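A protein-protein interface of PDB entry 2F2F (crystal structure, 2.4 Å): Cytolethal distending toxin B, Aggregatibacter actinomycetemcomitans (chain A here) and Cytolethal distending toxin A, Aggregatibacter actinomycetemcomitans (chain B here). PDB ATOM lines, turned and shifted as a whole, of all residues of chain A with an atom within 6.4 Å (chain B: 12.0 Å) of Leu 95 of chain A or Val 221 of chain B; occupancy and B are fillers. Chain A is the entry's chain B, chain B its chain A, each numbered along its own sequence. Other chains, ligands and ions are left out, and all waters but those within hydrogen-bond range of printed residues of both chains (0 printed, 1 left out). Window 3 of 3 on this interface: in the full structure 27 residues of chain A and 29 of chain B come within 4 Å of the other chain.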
ATOM      1  N   VAL A  49      12.403  11.765  17.912  1.00  0.00           N
ATOM      2  CA  VAL A  49      13.816  11.812  18.244  1.00  0.00           C
ATOM      3  C   VAL A  49      14.490  13.052  17.710  1.00  0.00           C
ATOM      4  O   VAL A  49      15.241  13.701  18.427  1.00  0.00           O
ATOM      5  CB  VAL A  49      14.559  10.579  17.768  1.00  0.00           C
ATOM      6  CG1 VAL A  49      16.044  10.770  18.019  1.00  0.00           C
ATOM      7  CG2 VAL A  49      14.060   9.356  18.537  1.00  0.00           C
ATOM      8  N   ARG A  50      14.228  13.385  16.451  1.00  0.00           N
ATOM      9  CA  ARG A  50      14.826  14.577  15.849  1.00  0.00           C
ATOM     10  C   ARG A  50      14.504  15.823  16.665  1.00  0.00           C
ATOM     11  O   ARG A  50      15.334  16.716  16.808  1.00  0.00           O
ATOM     12  CB  ARG A  50      14.322  14.772  14.424  1.00  0.00           C
ATOM     13  CG  ARG A  50      14.842  13.755  13.467  1.00  0.00           C
ATOM     14  CD  ARG A  50      14.394  14.029  12.038  1.00  0.00           C
ATOM     15  NE  ARG A  50      15.248  15.025  11.423  1.00  0.00           N
ATOM     16  CZ  ARG A  50      16.084  14.785  10.422  1.00  0.00           C
ATOM     17  NH1 ARG A  50      16.177  13.571   9.908  1.00  0.00           N
ATOM     18  NH2 ARG A  50      16.834  15.763   9.932  1.00  0.00           N
ATOM     19  N   LEU A  53      16.573  16.168  20.009  1.00  0.00           N
ATOM     20  CA  LEU A  53      17.967  16.533  19.788  1.00  0.00           C
ATOM     21  C   LEU A  53      18.223  17.955  19.253  1.00  0.00           C
ATOM     22  O   LEU A  53      19.376  18.397  19.186  1.00  0.00           O
ATOM     23  CB  LEU A  53      18.603  15.531  18.814  1.00  0.00           C
ATOM     24  CG  LEU A  53      18.631  14.058  19.235  1.00  0.00           C
ATOM     25  CD1 LEU A  53      18.936  13.187  18.024  1.00  0.00           C
ATOM     26  CD2 LEU A  53      19.672  13.862  20.334  1.00  0.00           C
ATOM     27  N   SER A  54      17.161  18.659  18.864  1.00  0.00           N
ATOM     28  CA  SER A  54      17.286  19.999  18.288  1.00  0.00           C
ATOM     29  C   SER A  54      17.098  21.185  19.230  1.00  0.00           C
ATOM     30  O   SER A  54      16.671  21.043  20.375  1.00  0.00           O
ATOM     31  CB  SER A  54      16.300  20.149  17.131  1.00  0.00           C
ATOM     32  OG  SER A  54      15.028  20.480  17.650  1.00  0.00           O
ATOM     33  N   TRP A  93      24.728   9.794  12.282  1.00  0.00           N
ATOM     34  CA  TRP A  93      23.439  10.124  11.688  1.00  0.00           C
ATOM     35  C   TRP A  93      23.373  11.619  11.423  1.00  0.00           C
ATOM     36  O   TRP A  93      23.455  12.419  12.342  1.00  0.00           O
ATOM     37  CB  TRP A  93      22.317   9.728  12.640  1.00  0.00           C
ATOM     38  CG  TRP A  93      20.934  10.020  12.143  1.00  0.00           C
ATOM     39  CD1 TRP A  93      20.500  10.004  10.840  1.00  0.00           C
ATOM     40  CD2 TRP A  93      19.775  10.272  12.951  1.00  0.00           C
ATOM     41  NE1 TRP A  93      19.143  10.223  10.799  1.00  0.00           N
ATOM     42  CE2 TRP A  93      18.673  10.390  12.076  1.00  0.00           C
ATOM     43  CE3 TRP A  93      19.561  10.408  14.331  1.00  0.00           C
ATOM     44  CZ2 TRP A  93      17.368  10.638  12.535  1.00  0.00           C
ATOM     45  CZ3 TRP A  93      18.260  10.649  14.784  1.00  0.00           C
ATOM     46  CH2 TRP A  93      17.180  10.762  13.883  1.00  0.00           C
ATOM     47  N   ASN A  94      23.187  11.982  10.164  1.00  0.00           N
ATOM     48  CA  ASN A  94      23.123  13.384   9.784  1.00  0.00           C
ATOM     49  C   ASN A  94      21.696  13.942   9.859  1.00  0.00           C
ATOM     50  O   ASN A  94      20.837  13.652   9.019  1.00  0.00           O
ATOM     51  CB  ASN A  94      23.684  13.555   8.369  1.00  0.00           C
ATOM     52  CG  ASN A  94      23.751  15.005   7.939  1.00  0.00           C
ATOM     53  OD1 ASN A  94      23.336  15.901   8.665  1.00  0.00           O
ATOM     54  ND2 ASN A  94      24.279  15.242   6.741  1.00  0.00           N
ATOM     55  N   LEU A  95      21.461  14.738  10.889  1.00  0.00           N
ATOM     56  CA  LEU A  95      20.174  15.379  11.112  1.00  0.00           C
ATOM     57  C   LEU A  95      19.936  16.555  10.163  1.00  0.00           C
ATOM     58  O   LEU A  95      18.867  17.148  10.175  1.00  0.00           O
ATOM     59  CB  LEU A  95      20.111  15.882  12.543  1.00  0.00           C
ATOM     60  CG  LEU A  95      20.187  14.833  13.634  1.00  0.00           C
ATOM     61  CD1 LEU A  95      20.207  15.550  14.973  1.00  0.00           C
ATOM     62  CD2 LEU A  95      18.988  13.897  13.560  1.00  0.00           C
ATOM     63  N   GLY A  96      20.939  16.908   9.365  1.00  0.00           N
ATOM     64  CA  GLY A  96      20.796  18.032   8.461  1.00  0.00           C
ATOM     65  C   GLY A  96      21.025  17.590   7.049  1.00  0.00           C
ATOM     66  O   GLY A  96      20.977  16.403   6.784  1.00  0.00           O
ATOM     67  N   THR A  97      21.278  18.526   6.144  1.00  0.00           N
ATOM     68  CA  THR A  97      21.496  18.189   4.750  1.00  0.00           C
ATOM     69  C   THR A  97      22.951  17.824   4.484  1.00  0.00           C
ATOM     70  O   THR A  97      23.819  18.028   5.328  1.00  0.00           O
ATOM     71  CB  THR A  97      21.078  19.367   3.837  1.00  0.00           C
ATOM     72  OG1 THR A  97      21.959  20.470   4.036  1.00  0.00           O
ATOM     73  CG2 THR A  97      19.661  19.833   4.175  1.00  0.00           C
ATOM     74  N   ARG A 100      24.850  21.075   4.488  1.00  0.00           N
ATOM     75  CA  ARG A 100      24.921  21.673   5.816  1.00  0.00           C
ATOM     76  C   ARG A 100      24.587  20.602   6.849  1.00  0.00           C
ATOM     77  O   ARG A 100      23.482  20.554   7.393  1.00  0.00           O
ATOM     78  CB  ARG A 100      23.910  22.818   5.926  1.00  0.00           C
ATOM     79  CG  ARG A 100      24.050  23.873   4.833  1.00  0.00           C
ATOM     80  CD  ARG A 100      24.878  25.051   5.307  1.00  0.00           C
ATOM     81  NE  ARG A 100      25.002  25.101   6.761  1.00  0.00           N
ATOM     82  CZ  ARG A 100      25.454  26.150   7.441  1.00  0.00           C
ATOM     83  NH1 ARG A 100      25.525  26.103   8.770  1.00  0.00           N
ATOM     84  NH2 ARG A 100      25.822  27.242   6.786  1.00  0.00           N
ATOM     85  N   PRO A 101      25.571  19.749   7.158  1.00  0.00           N
ATOM     86  CA  PRO A 101      25.357  18.679   8.129  1.00  0.00           C
ATOM     87  C   PRO A 101      25.125  19.063   9.575  1.00  0.00           C
ATOM     88  O   PRO A 101      25.541  20.111  10.036  1.00  0.00           O
ATOM     89  CB  PRO A 101      26.596  17.804   7.974  1.00  0.00           C
ATOM     90  CG  PRO A 101      27.615  18.672   7.335  1.00  0.00           C
ATOM     91  CD  PRO A 101      26.916  19.720   6.568  1.00  0.00           C
ATOM     92  N   ASN A 102      24.435  18.183  10.282  1.00  0.00           N
ATOM     93  CA  ASN A 102      24.162  18.345  11.689  1.00  0.00           C
ATOM     94  C   ASN A 102      24.251  16.926  12.234  1.00  0.00           C
ATOM     95  O   ASN A 102      23.263  16.199  12.253  1.00  0.00           O
ATOM     96  CB  ASN A 102      22.769  18.896  11.899  1.00  0.00           C
ATOM     97  CG  ASN A 102      22.471  19.094  13.344  1.00  0.00           C
ATOM     98  OD1 ASN A 102      22.413  20.190  13.826  1.00  0.00           O
ATOM     99  ND2 ASN A 102      22.307  18.015  14.044  1.00  0.00           N
ATOM    100  N   MET A 103      25.426  16.556  12.731  1.00  0.00           N
ATOM    101  CA  MET A 103      25.670  15.198  13.184  1.00  0.00           C
ATOM    102  C   MET A 103      25.548  14.790  14.640  1.00  0.00           C
ATOM    103  O   MET A 103      25.670  15.592  15.560  1.00  0.00           O
ATOM    104  CB  MET A 103      27.042  14.768  12.676  1.00  0.00           C
ATOM    105  CG  MET A 103      27.361  15.288  11.295  1.00  0.00           C
ATOM    106  SD  MET A 103      26.593  14.298  10.022  1.00  0.00           S
ATOM    107  CE  MET A 103      27.062  12.630  10.539  1.00  0.00           C
ATOM    108  N   VAL A 104      25.325  13.497  14.820  1.00  0.00           N
ATOM    109  CA  VAL A 104      25.232  12.891  16.135  1.00  0.00           C
ATOM    110  C   VAL A 104      25.737  11.474  15.925  1.00  0.00           C
ATOM    111  O   VAL A 104      25.755  10.971  14.798  1.00  0.00           O
ATOM    112  CB  VAL A 104      23.773  12.810  16.680  1.00  0.00           C
ATOM    113  CG1 VAL A 104      23.206  14.199  16.892  1.00  0.00           C
ATOM    114  CG2 VAL A 104      22.903  12.014  15.732  1.00  0.00           C
ATOM    115  N   VAL A 123      22.182   8.214  21.693  1.00  0.00           N
ATOM    116  CA  VAL A 123      22.518   9.180  20.643  1.00  0.00           C
ATOM    117  C   VAL A 123      23.366  10.240  21.332  1.00  0.00           C
ATOM    118  O   VAL A 123      23.011  10.733  22.405  1.00  0.00           O
ATOM    119  CB  VAL A 123      21.242   9.825  20.022  1.00  0.00           C
ATOM    120  CG1 VAL A 123      21.615  10.682  18.830  1.00  0.00           C
ATOM    121  CG2 VAL A 123      20.261   8.731  19.586  1.00  0.00           C
ATOM    122  N   ARG A 125      25.991  13.806  20.589  1.00  0.00           N
ATOM    123  CA  ARG A 125      26.509  14.802  19.653  1.00  0.00           C
ATOM    124  C   ARG A 125      28.019  14.590  19.607  1.00  0.00           C
ATOM    125  O   ARG A 125      28.657  14.829  18.582  1.00  0.00           O
ATOM    126  CB  ARG A 125      26.188  16.232  20.116  1.00  0.00           C
ATOM    127  CG  ARG A 125      24.839  16.388  20.805  1.00  0.00           C
ATOM    128  CD  ARG A 125      23.825  17.199  19.980  1.00  0.00           C
ATOM    129  NE  ARG A 125      24.143  17.300  18.555  1.00  0.00           N
ATOM    130  CZ  ARG A 125      23.282  17.695  17.623  1.00  0.00           C
ATOM    131  NH1 ARG A 125      22.042  18.030  17.954  1.00  0.00           N
ATOM    132  NH2 ARG A 125      23.657  17.763  16.350  1.00  0.00           N
ATOM    133  N   PRO B  70      17.699  27.475   9.209  1.00  0.00           N
ATOM    134  CA  PRO B  70      18.483  28.131  10.292  1.00  0.00           C
ATOM    135  C   PRO B  70      18.478  27.329  11.600  1.00  0.00           C
ATOM    136  O   PRO B  70      17.895  26.238  11.669  1.00  0.00           O
ATOM    137  CB  PRO B  70      17.922  29.532  10.508  1.00  0.00           C
ATOM    138  CG  PRO B  70      17.059  29.770   9.264  1.00  0.00           C
ATOM    139  CD  PRO B  70      16.814  28.439   8.524  1.00  0.00           C
ATOM    140  N   SER B  71      19.113  27.880  12.635  1.00  0.00           N
ATOM    141  CA  SER B  71      19.227  27.204  13.930  1.00  0.00           C
ATOM    142  C   SER B  71      18.436  27.843  15.064  1.00  0.00           C
ATOM    143  O   SER B  71      18.349  27.293  16.164  1.00  0.00           O
ATOM    144  CB  SER B  71      20.695  27.180  14.356  1.00  0.00           C
ATOM    145  OG  SER B  71      21.126  28.493  14.705  1.00  0.00           O
ATOM    146  N   GLU B  72      17.832  28.991  14.793  1.00  0.00           N
ATOM    147  CA  GLU B  72      17.064  29.672  15.806  1.00  0.00           C
ATOM    148  C   GLU B  72      15.588  29.269  15.748  1.00  0.00           C
ATOM    149  O   GLU B  72      14.954  29.112  16.788  1.00  0.00           O
ATOM    150  CB  GLU B  72      17.206  31.181  15.627  1.00  0.00           C
ATOM    151  CG  GLU B  72      16.672  31.994  16.791  1.00  0.00           C
ATOM    152  CD  GLU B  72      17.537  31.871  18.046  1.00  0.00           C
ATOM    153  OE1 GLU B  72      18.118  32.893  18.480  1.00  0.00           O
ATOM    154  OE2 GLU B  72      17.646  30.761  18.614  1.00  0.00           O
ATOM    155  N   PRO B  73      15.031  29.073  14.535  1.00  0.00           N
ATOM    156  CA  PRO B  73      13.621  28.687  14.358  1.00  0.00           C
ATOM    157  C   PRO B  73      13.195  27.505  15.225  1.00  0.00           C
ATOM    158  O   PRO B  73      12.131  27.532  15.846  1.00  0.00           O
ATOM    159  CB  PRO B  73      13.530  28.353  12.874  1.00  0.00           C
ATOM    160  CG  PRO B  73      14.580  29.144  12.249  1.00  0.00           C
ATOM    161  CD  PRO B  73      15.704  29.230  13.233  1.00  0.00           C
ATOM    162  N   SER B  74      14.049  26.483  15.282  1.00  0.00           N
ATOM    163  CA  SER B  74      13.776  25.287  16.071  1.00  0.00           C
ATOM    164  C   SER B  74      13.499  25.623  17.520  1.00  0.00           C
ATOM    165  O   SER B  74      12.982  24.801  18.270  1.00  0.00           O
ATOM    166  CB  SER B  74      14.962  24.332  16.000  1.00  0.00           C
ATOM    167  OG  SER B  74      16.132  24.932  16.538  1.00  0.00           O
ATOM    168  N   ASN B  75      13.848  26.832  17.930  1.00  0.00           N
ATOM    169  CA  ASN B  75      13.622  27.219  19.310  1.00  0.00           C
ATOM    170  C   ASN B  75      12.219  27.740  19.563  1.00  0.00           C
ATOM    171  O   ASN B  75      11.843  27.962  20.711  1.00  0.00           O
ATOM    172  CB  ASN B  75      14.651  28.265  19.737  1.00  0.00           C
ATOM    173  CG  ASN B  75      16.038  27.677  19.854  1.00  0.00           C
ATOM    174  OD1 ASN B  75      16.307  26.903  20.771  1.00  0.00           O
ATOM    175  ND2 ASN B  75      16.916  28.020  18.924  1.00  0.00           N
ATOM    176  N   GLU B 217       8.420  30.070   8.185  1.00  0.00           N
ATOM    177  CA  GLU B 217       8.747  29.341   6.982  1.00  0.00           C
ATOM    178  C   GLU B 217       9.663  28.224   7.471  1.00  0.00           C
ATOM    179  O   GLU B 217      10.447  28.426   8.399  1.00  0.00           O
ATOM    180  CB  GLU B 217       9.467  30.248   5.997  1.00  0.00           C
ATOM    181  CG  GLU B 217       8.496  30.985   5.089  1.00  0.00           C
ATOM    182  CD  GLU B 217       9.177  31.637   3.907  1.00  0.00           C
ATOM    183  OE1 GLU B 217      10.295  32.170   4.092  1.00  0.00           O
ATOM    184  OE2 GLU B 217       8.589  31.614   2.797  1.00  0.00           O
ATOM    185  N   ALA B 218       9.541  27.047   6.872  1.00  0.00           N
ATOM    186  CA  ALA B 218      10.318  25.894   7.291  1.00  0.00           C
ATOM    187  C   ALA B 218      11.255  25.460   6.211  1.00  0.00           C
ATOM    188  O   ALA B 218      10.920  25.521   5.041  1.00  0.00           O
ATOM    189  CB  ALA B 218       9.385  24.756   7.647  1.00  0.00           C
ATOM    190  N   THR B 219      12.434  25.006   6.604  1.00  0.00           N
ATOM    191  CA  THR B 219      13.417  24.559   5.628  1.00  0.00           C
ATOM    192  C   THR B 219      13.539  23.044   5.732  1.00  0.00           C
ATOM    193  O   THR B 219      13.690  22.512   6.829  1.00  0.00           O
ATOM    194  CB  THR B 219      14.792  25.202   5.901  1.00  0.00           C
ATOM    195  OG1 THR B 219      14.651  26.630   5.951  1.00  0.00           O
ATOM    196  CG2 THR B 219      15.789  24.831   4.809  1.00  0.00           C
ATOM    197  N   ALA B 220      13.435  22.352   4.604  1.00  0.00           N
ATOM    198  CA  ALA B 220      13.553  20.906   4.608  1.00  0.00           C
ATOM    199  C   ALA B 220      15.004  20.502   4.950  1.00  0.00           C
ATOM    200  O   ALA B 220      15.959  20.987   4.334  1.00  0.00           O
ATOM    201  CB  ALA B 220      13.157  20.351   3.241  1.00  0.00           C
ATOM    202  N   VAL B 221      15.164  19.583   5.902  1.00  0.00           N
ATOM    203  CA  VAL B 221      16.496  19.131   6.294  1.00  0.00           C
ATOM    204  C   VAL B 221      16.792  17.683   5.885  1.00  0.00           C
ATOM    205  O   VAL B 221      17.644  17.021   6.472  1.00  0.00           O
ATOM    206  CB  VAL B 221      16.737  19.309   7.814  1.00  0.00           C
ATOM    207  CG1 VAL B 221      16.846  20.785   8.131  1.00  0.00           C
ATOM    208  CG2 VAL B 221      15.639  18.667   8.631  1.00  0.00           C
ATOM    209  N   ASN B 222      16.067  17.191   4.889  1.00  0.00           N
ATOM    210  CA  ASN B 222      16.260  15.837   4.383  1.00  0.00           C
ATOM    211  C   ASN B 222      17.538  15.764   3.537  1.00  0.00           C
ATOM    212  O   ASN B 222      18.060  14.644   3.309  1.00  0.00           O
ATOM    213  CB  ASN B 222      15.057  15.434   3.526  1.00  0.00           C
ATOM    214  CG  ASN B 222      14.822  16.388   2.369  1.00  0.00           C
ATOM    215  OD1 ASN B 222      14.676  17.601   2.558  1.00  0.00           O
ATOM    216  ND2 ASN B 222      14.792  15.847   1.167  1.00  0.00           N
ATOM    217  OXT ASN B 222      18.005  16.838   3.094  1.00  0.00           O
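The backbone carbonyl oxygen of Leu 95 of chain A sits at hydrogen-bond distance from the guanidinium group of Arg 50 of chain A (2.5 Å).
N of Gly 96 of chain A lies within hydrogen-bond range of OD1 of Asn 94 of chain A.
ND2 of Asn 94 of chain A lies within hydrogen-bond range of O of Thr 97 of chain A (3.2 Å).
The backbone NH of Leu 95 of chain A lies within hydrogen-bond range of the backbone carbonyl oxygen of Asn 102 of chain A, at 2.7 Å.
The backbone NH (N) of Arg 100 of chain A lies within hydrogen-bond range of the side-chain hydroxyl (OG1) of Thr 97 of chain A.
Among the printed residues, merely in contact across the chains: Arg 50 of chain A with Val 221 of chain B (3.4 Å), Leu 95 of chain A with Val 221 of chain B (3.8 Å), Thr 97 of chain A with Ala 220 of chain B (3.9 Å), Thr 97 of chain A with Val 221 of chain B (3.9 Å) and Thr 97 of chain A with Asn 222 of chain B (3.6 Å).
The backbone carbonyl oxygen (O) of Gly 96 of chain A lies close to the backbone carbonyl oxygen (O) of Val 221 of chain B (3.4 Å).
Leu 95 of chain A touches just one residue of chain B: Val 221 (3.8 Å).
Of the printed residues of chain A, Val 221 of chain B touches Arg 50, Leu 95, Gly 96 and Thr 97.
Arg 50 of chain A touches just one residue of chain B: Val 221 (3.4 Å).
No residue of chain B comes within 4 Å of Leu 53 of chain A.
No residue of chain B comes within 4 Å of Asn 94 of chain A.
Gly 96 of chain A touches just one residue of chain B: Val 221.
Of chain B, only Ala 220 (3.9 Å), Val 221 (3.9 Å) and Asn 222 (3.6 Å) come within 4 Å of Thr 97 of chain A.
No residue of chain B comes within 4 Å of Asn 102 of chain A.
No residue of chain B comes within 4 Å of Val 104 of chain A.
Of the printed residues of chain A, Asn 222 of chain B touches Thr 97 (3.6 Å).
Of the printed residues of chain A, Ala 220 of chain B touches Thr 97.
The nearest residue of chain B that does not touch Leu 95 of chain A is Asn 222 of chain B (6.0 Å).
The nearest residue of chain A that does not touch Val 221 of chain B is Asn 94 of chain A (5.3 Å).
Of the 16 printed residues of chain A, 4 touch a printed residue of chain B.
Of the 12 printed residues of chain B, 3 touch a printed residue of chain A.
Among the printed residues, 6 pairs touch across the chains.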
